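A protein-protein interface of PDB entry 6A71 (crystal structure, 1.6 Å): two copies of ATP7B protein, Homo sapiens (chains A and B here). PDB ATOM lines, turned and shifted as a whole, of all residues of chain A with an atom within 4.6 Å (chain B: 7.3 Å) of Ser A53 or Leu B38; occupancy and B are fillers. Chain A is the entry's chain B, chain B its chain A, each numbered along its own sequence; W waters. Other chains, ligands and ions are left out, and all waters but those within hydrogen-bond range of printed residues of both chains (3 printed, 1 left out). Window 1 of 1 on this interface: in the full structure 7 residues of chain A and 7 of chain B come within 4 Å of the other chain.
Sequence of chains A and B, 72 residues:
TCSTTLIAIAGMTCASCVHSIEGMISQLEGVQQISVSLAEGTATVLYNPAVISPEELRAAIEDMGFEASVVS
The side-chain carboxylate (OE1) of Glu A56 lies within hydrogen-bond range of the side-chain hydroxyl (OG) of Ser A53 (2.7 Å).
The side-chain hydroxyl (OG) of Ser A53 lies close to the backbone NH (N) of Glu A55, 3.5 Å away.
Ser A53 touches Leu B38 (OG to CD2, 3.6 Å).
Glu A55 touches Ala B15.
CD of Glu A55 touches CD2 of Leu B38, 3.6 Å away.
Glu A56 touches Ala B15.
Glu A56 touches Val B18.
Ser A53 touches just one residue of chain B: Leu B38 (3.6 Å).
Pro A54 touches none of the printed residues of chain B.
Printed residues of chain B within 4 Å of Glu A56: Ala B15 (3.8 Å) and Val B18 (3.3 Å).
Of the printed residues of chain A, Ala B15 touches Glu A55 (3.7 Å) and Glu A56 (3.8 Å).
The nearest residue of chain B that does not touch Ser A53 is Ala B39 (5.0 Å).
The nearest residue of chain A that does not touch Leu B38 is Glu A56 (4.4 Å).
Of the 7 printed residues of chain A, 3 touch a printed residue of chain B.
Among the printed residues, 5 pairs touch across the chains.
Among the printed residues, no Asp or Glu carboxylate lies within 4 Å of a Lys or Arg side-chain nitrogen of the other chain.
No position is printed for both chains.
Of the 5 pairs that touch across the chains among the printed residues, none has its exchanged pair printed and touching as well.
Water W2 lies within hydrogen-bond range of the side-chain carboxylate of Glu A56 (2.6 Å), the backbone carbonyl oxygen of Val B36 (2.9 Å) and the backbone NH of Leu B38 (3.0 Å).
Water W1 lies within hydrogen-bond range of the side-chain carboxylate (OE2) of Glu A55 and the backbone carbonyl oxygen (O) of Thr B13.
Water W3 lies within hydrogen-bond range of the backbone NH (N) of Ala B39 (3.0 Å), the backbone NH (N) of Leu B38 (3.2 Å), the backbone carbonyl oxygen (O) of Ile A52 (3.3 Å) and the side-chain hydroxyl (OG) of Ser B37 (3.5 Å).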
ATOM      1  N   TYR A  47     -12.770  18.788 -19.032  1.00  0.00           N
ATOM      2  CA  TYR A  47     -11.654  19.635 -19.583  1.00  0.00           C
ATOM      3  C   TYR A  47     -11.148  19.091 -20.921  1.00  0.00           C
ATOM      4  O   TYR A  47     -11.321  17.909 -21.247  1.00  0.00           O
ATOM      5  CB  TYR A  47     -10.514  19.713 -18.527  1.00  0.00           C
ATOM      6  CG  TYR A  47      -9.792  18.407 -18.375  1.00  0.00           C
ATOM      7  CD1 TYR A  47     -10.345  17.356 -17.605  1.00  0.00           C
ATOM      8  CD2 TYR A  47      -8.667  18.125 -19.105  1.00  0.00           C
ATOM      9  CE1 TYR A  47      -9.722  16.130 -17.533  1.00  0.00           C
ATOM     10  CE2 TYR A  47      -8.027  16.916 -19.032  1.00  0.00           C
ATOM     11  CZ  TYR A  47      -8.579  15.891 -18.270  1.00  0.00           C
ATOM     12  OH  TYR A  47      -8.035  14.616 -18.245  1.00  0.00           O
ATOM     13  N   ILE A  52      -5.222  21.463 -21.134  1.00  0.00           N
ATOM     14  CA  ILE A  52      -5.006  21.430 -19.692  1.00  0.00           C
ATOM     15  C   ILE A  52      -5.098  19.978 -19.218  1.00  0.00           C
ATOM     16  O   ILE A  52      -5.728  19.188 -19.877  1.00  0.00           O
ATOM     17  CB  ILE A  52      -5.928  22.411 -18.946  1.00  0.00           C
ATOM     18  CG1 ILE A  52      -5.488  22.680 -17.482  1.00  0.00           C
ATOM     19  CG2 ILE A  52      -7.360  21.903 -18.985  1.00  0.00           C
ATOM     20  CD1 ILE A  52      -6.199  23.814 -16.807  1.00  0.00           C
ATOM     21  N   SER A  53      -4.429  19.695 -18.120  1.00  0.00           N
ATOM     22  CA  SER A  53      -4.278  18.363 -17.526  1.00  0.00           C
ATOM     23  C   SER A  53      -4.826  18.270 -16.120  1.00  0.00           C
ATOM     24  O   SER A  53      -4.940  19.272 -15.426  1.00  0.00           O
ATOM     25  CB  SER A  53      -2.811  17.986 -17.496  1.00  0.00           C
ATOM     26  OG  SER A  53      -2.100  18.813 -16.585  1.00  0.00           O
ATOM     27  N   PRO A  54      -5.156  17.052 -15.669  1.00  0.00           N
ATOM     28  CA  PRO A  54      -5.476  16.859 -14.273  1.00  0.00           C
ATOM     29  C   PRO A  54      -4.389  17.370 -13.313  1.00  0.00           C
ATOM     30  O   PRO A  54      -4.720  17.954 -12.284  1.00  0.00           O
ATOM     31  CB  PRO A  54      -5.657  15.362 -14.164  1.00  0.00           C
ATOM     32  CG  PRO A  54      -6.147  14.975 -15.542  1.00  0.00           C
ATOM     33  CD  PRO A  54      -5.351  15.835 -16.458  1.00  0.00           C
ATOM     34  N   GLU A  55      -3.110  17.186 -13.679  1.00  0.00           N
ATOM     35  CA  GLU A  55      -1.993  17.643 -12.863  1.00  0.00           C
ATOM     36  C   GLU A  55      -2.038  19.159 -12.688  1.00  0.00           C
ATOM     37  O   GLU A  55      -1.884  19.657 -11.579  1.00  0.00           O
ATOM     38  CB  GLU A  55      -0.652  17.241 -13.496  1.00  0.00           C
ATOM     39  CG  GLU A  55      -0.388  15.747 -13.461  1.00  0.00           C
ATOM     40  CD  GLU A  55      -0.868  14.918 -14.677  1.00  0.00           C
ATOM     41  OE1 GLU A  55      -1.870  15.255 -15.422  1.00  0.00           O
ATOM     42  OE2 GLU A  55      -0.198  13.838 -14.848  1.00  0.00           O
ATOM     43  N   GLU A  56      -2.283  19.873 -13.782  1.00  0.00           N
ATOM     44  CA  GLU A  56      -2.389  21.319 -13.718  1.00  0.00           C
ATOM     45  C   GLU A  56      -3.603  21.772 -12.899  1.00  0.00           C
ATOM     46  O   GLU A  56      -3.545  22.758 -12.172  1.00  0.00           O
ATOM     47  CB  GLU A  56      -2.434  21.899 -15.125  1.00  0.00           C
ATOM     48  CG  GLU A  56      -1.086  21.813 -15.854  1.00  0.00           C
ATOM     49  CD  GLU A  56      -1.271  21.986 -17.324  1.00  0.00           C
ATOM     50  OE1 GLU A  56      -1.555  21.009 -17.989  1.00  0.00           O
ATOM     51  OE2 GLU A  56      -1.117  23.127 -17.818  1.00  0.00           O
ATOM     52  N   LEU A  57      -4.746  21.085 -13.054  1.00  0.00           N
ATOM     53  CA  LEU A  57      -5.950  21.392 -12.284  1.00  0.00           C
ATOM     54  C   LEU A  57      -5.707  21.251 -10.788  1.00  0.00           C
ATOM     55  O   LEU A  57      -6.018  22.128  -9.982  1.00  0.00           O
ATOM     56  CB  LEU A  57      -7.110  20.525 -12.776  1.00  0.00           C
ATOM     57  CG  LEU A  57      -7.600  20.874 -14.180  1.00  0.00           C
ATOM     58  CD1 LEU A  57      -8.386  19.734 -14.857  1.00  0.00           C
ATOM     59  CD2 LEU A  57      -8.334  22.196 -14.197  1.00  0.00           C
ATOM     60  N   ILE B   9       7.301  17.023 -27.235  1.00  0.00           N
ATOM     61  CA  ILE B   9       8.151  17.217 -26.112  1.00  0.00           C
ATOM     62  C   ILE B   9       8.113  15.963 -25.259  1.00  0.00           C
ATOM     63  O   ILE B   9       7.035  15.617 -24.748  1.00  0.00           O
ATOM     64  CB  ILE B   9       7.770  18.431 -25.262  1.00  0.00           C
ATOM     65  CG1 ILE B   9       7.718  19.698 -26.105  1.00  0.00           C
ATOM     66  CG2 ILE B   9       8.766  18.607 -24.104  1.00  0.00           C
ATOM     67  CD1 ILE B   9       7.164  20.911 -25.388  1.00  0.00           C
ATOM     68  N   GLY B  11       9.257  13.703 -21.929  1.00  0.00           N
ATOM     69  CA  GLY B  11       9.737  13.762 -20.566  1.00  0.00           C
ATOM     70  C   GLY B  11       8.992  14.666 -19.599  1.00  0.00           C
ATOM     71  O   GLY B  11       9.408  14.823 -18.468  1.00  0.00           O
ATOM     72  N   MET B  12       7.926  15.333 -20.056  1.00  0.00           N
ATOM     73  CA  MET B  12       7.142  16.181 -19.126  1.00  0.00           C
ATOM     74  C   MET B  12       6.281  15.336 -18.206  1.00  0.00           C
ATOM     75  O   MET B  12       5.500  14.530 -18.679  1.00  0.00           O
ATOM     76  CB  MET B  12       6.247  17.182 -19.841  1.00  0.00           C
ATOM     77  CG  MET B  12       6.926  18.034 -20.909  1.00  0.00           C
ATOM     78  SD  MET B  12       5.755  19.166 -21.704  1.00  0.00           S
ATOM     79  CE  MET B  12       4.808  18.023 -22.714  1.00  0.00           C
ATOM     80  N   THR B  13       6.509  15.490 -16.902  1.00  0.00           N
ATOM     81  CA  THR B  13       5.827  14.639 -15.889  1.00  0.00           C
ATOM     82  C   THR B  13       5.250  15.409 -14.728  1.00  0.00           C
ATOM     83  O   THR B  13       4.841  14.809 -13.703  1.00  0.00           O
ATOM     84  CB  THR B  13       6.820  13.530 -15.397  1.00  0.00           C
ATOM     85  OG1 THR B  13       8.046  14.123 -15.040  1.00  0.00           O
ATOM     86  CG2 THR B  13       7.103  12.513 -16.493  1.00  0.00           C
ATOM     87  N   CYS B  14       5.149  16.730 -14.854  1.00  0.00           N
ATOM     88  CA  CYS B  14       4.592  17.568 -13.787  1.00  0.00           C
ATOM     89  C   CYS B  14       3.987  18.840 -14.339  1.00  0.00           C
ATOM     90  O   CYS B  14       4.376  19.353 -15.433  1.00  0.00           O
ATOM     91  CB  CYS B  14       5.652  17.893 -12.755  1.00  0.00           C
ATOM     92  SG  CYS B  14       6.964  18.957 -13.467  1.00  0.00           S
ATOM     93  N   ALA B  15       3.075  19.406 -13.559  1.00  0.00           N
ATOM     94  CA  ALA B  15       2.493  20.708 -13.857  1.00  0.00           C
ATOM     95  C   ALA B  15       3.514  21.843 -13.843  1.00  0.00           C
ATOM     96  O   ALA B  15       3.426  22.767 -14.672  1.00  0.00           O
ATOM     97  CB  ALA B  15       1.347  21.007 -12.889  1.00  0.00           C
ATOM     98  N   SER B  16       4.444  21.819 -12.884  1.00  0.00           N
ATOM     99  CA  SER B  16       5.480  22.846 -12.774  1.00  0.00           C
ATOM    100  C   SER B  16       6.229  23.029 -14.071  1.00  0.00           C
ATOM    101  O   SER B  16       6.429  24.151 -14.512  1.00  0.00           O
ATOM    102  CB  SER B  16       6.466  22.504 -11.665  1.00  0.00           C
ATOM    103  OG  SER B  16       7.487  23.496 -11.549  1.00  0.00           O
ATOM    104  N   CYS B  17       6.638  21.919 -14.669  1.00  0.00           N
ATOM    105  CA  CYS B  17       7.374  21.971 -15.902  1.00  0.00           C
ATOM    106  C   CYS B  17       6.557  22.474 -17.071  1.00  0.00           C
ATOM    107  O   CYS B  17       7.086  23.228 -17.913  1.00  0.00           O
ATOM    108  CB  CYS B  17       7.969  20.623 -16.275  1.00  0.00           C
ATOM    109  SG  CYS B  17       9.300  20.071 -15.168  1.00  0.00           S
ATOM    110  N   VAL B  18       5.298  22.090 -17.145  1.00  0.00           N
ATOM    111  CA  VAL B  18       4.398  22.668 -18.171  1.00  0.00           C
ATOM    112  C   VAL B  18       4.411  24.206 -18.084  1.00  0.00           C
ATOM    113  O   VAL B  18       4.618  24.932 -19.105  1.00  0.00           O
ATOM    114  CB  VAL B  18       2.950  22.138 -18.049  1.00  0.00           C
ATOM    115  CG1 VAL B  18       2.003  22.860 -18.966  1.00  0.00           C
ATOM    116  CG2 VAL B  18       2.910  20.633 -18.272  1.00  0.00           C
ATOM    117  N   SER B  35       0.545  26.523 -26.236  1.00  0.00           N
ATOM    118  CA  SER B  35      -0.353  25.589 -25.505  1.00  0.00           C
ATOM    119  C   SER B  35       0.359  24.247 -25.367  1.00  0.00           C
ATOM    120  O   SER B  35       0.499  23.516 -26.354  1.00  0.00           O
ATOM    121  CB  SER B  35      -1.659  25.341 -26.250  1.00  0.00           C
ATOM    122  OG  SER B  35      -2.327  26.583 -26.432  1.00  0.00           O
ATOM    123  N   VAL B  36       0.744  23.893 -24.156  1.00  0.00           N
ATOM    124  CA  VAL B  36       1.395  22.581 -23.864  1.00  0.00           C
ATOM    125  C   VAL B  36       0.329  21.618 -23.413  1.00  0.00           C
ATOM    126  O   VAL B  36      -0.480  21.933 -22.509  1.00  0.00           O
ATOM    127  CB  VAL B  36       2.487  22.730 -22.822  1.00  0.00           C
ATOM    128  CG1 VAL B  36       3.023  21.353 -22.362  1.00  0.00           C
ATOM    129  CG2 VAL B  36       3.606  23.557 -23.394  1.00  0.00           C
ATOM    130  N   SER B  37       0.271  20.461 -24.087  1.00  0.00           N
ATOM    131  CA  SER B  37      -0.594  19.330 -23.685  1.00  0.00           C
ATOM    132  C   SER B  37       0.284  18.327 -22.956  1.00  0.00           C
ATOM    133  O   SER B  37       1.034  17.600 -23.587  1.00  0.00           O
ATOM    134  CB  SER B  37      -1.256  18.664 -24.862  1.00  0.00           C
ATOM    135  OG  SER B  37      -2.015  17.516 -24.428  1.00  0.00           O
ATOM    136  N   LEU B  38       0.163  18.260 -21.630  1.00  0.00           N
ATOM    137  CA  LEU B  38       0.889  17.245 -20.857  1.00  0.00           C
ATOM    138  C   LEU B  38       0.374  15.833 -21.305  1.00  0.00           C
ATOM    139  O   LEU B  38       1.164  14.899 -21.446  1.00  0.00           O
ATOM    140  CB  LEU B  38       0.731  17.531 -19.380  1.00  0.00           C
ATOM    141  CG  LEU B  38       1.400  16.617 -18.382  1.00  0.00           C
ATOM    142  CD1 LEU B  38       2.912  16.623 -18.540  1.00  0.00           C
ATOM    143  CD2 LEU B  38       1.020  16.994 -16.979  1.00  0.00           C
ATOM    144  N   ALA B  39      -0.921  15.699 -21.580  1.00  0.00           N
ATOM    145  CA  ALA B  39      -1.500  14.435 -22.061  1.00  0.00           C
ATOM    146  C   ALA B  39      -0.918  13.920 -23.328  1.00  0.00           C
ATOM    147  O   ALA B  39      -0.611  12.718 -23.424  1.00  0.00           O
ATOM    148  CB  ALA B  39      -3.018  14.547 -22.263  1.00  0.00           C
ATOM    149  N   GLU B  40      -0.763  14.797 -24.307  1.00  0.00           N
ATOM    150  CA  GLU B  40      -0.361  14.451 -25.662  1.00  0.00           C
ATOM    151  C   GLU B  40       1.157  14.544 -25.823  1.00  0.00           C
ATOM    152  O   GLU B  40       1.697  14.067 -26.824  1.00  0.00           O
ATOM    153  CB  GLU B  40      -1.097  15.346 -26.693  1.00  0.00           C
ATOM    154  CG  GLU B  40      -2.515  14.861 -26.983  1.00  0.00           C
ATOM    155  CD  GLU B  40      -3.571  15.947 -27.243  1.00  0.00           C
ATOM    156  OE1 GLU B  40      -3.297  16.882 -28.022  1.00  0.00           O
ATOM    157  OE2 GLU B  40      -4.707  15.821 -26.675  1.00  0.00           O
ATOM    158  N   GLY B  41       1.825  15.164 -24.848  1.00  0.00           N
ATOM    159  CA  GLY B  41       3.267  15.388 -24.935  1.00  0.00           C
ATOM    160  C   GLY B  41       3.647  16.312 -26.062  1.00  0.00           C
ATOM    161  O   GLY B  41       4.654  16.077 -26.783  1.00  0.00           O
ATOM    162  N   THR B  42       2.864  17.390 -26.232  1.00  0.00           N
ATOM    163  CA  THR B  42       3.144  18.327 -27.339  1.00  0.00           C
ATOM    164  C   THR B  42       2.992  19.768 -26.910  1.00  0.00           C
ATOM    165  O   THR B  42       2.358  20.031 -25.894  1.00  0.00           O
ATOM    166  CB  THR B  42       2.223  18.102 -28.530  1.00  0.00           C
ATOM    167  OG1 THR B  42       0.857  18.292 -28.111  1.00  0.00           O
ATOM    168  CG2 THR B  42       2.438  16.755 -29.101  1.00  0.00           C
HETATM  169  O   HOH W   1       2.520  13.637 -15.561  1.00  0.00           O
HETATM  170  O   HOH W   2      -1.714  20.300 -20.505  1.00  0.00           O
HETATM  171  O   HOH W   3      -2.958  17.794 -21.102  1.00  0.00           O
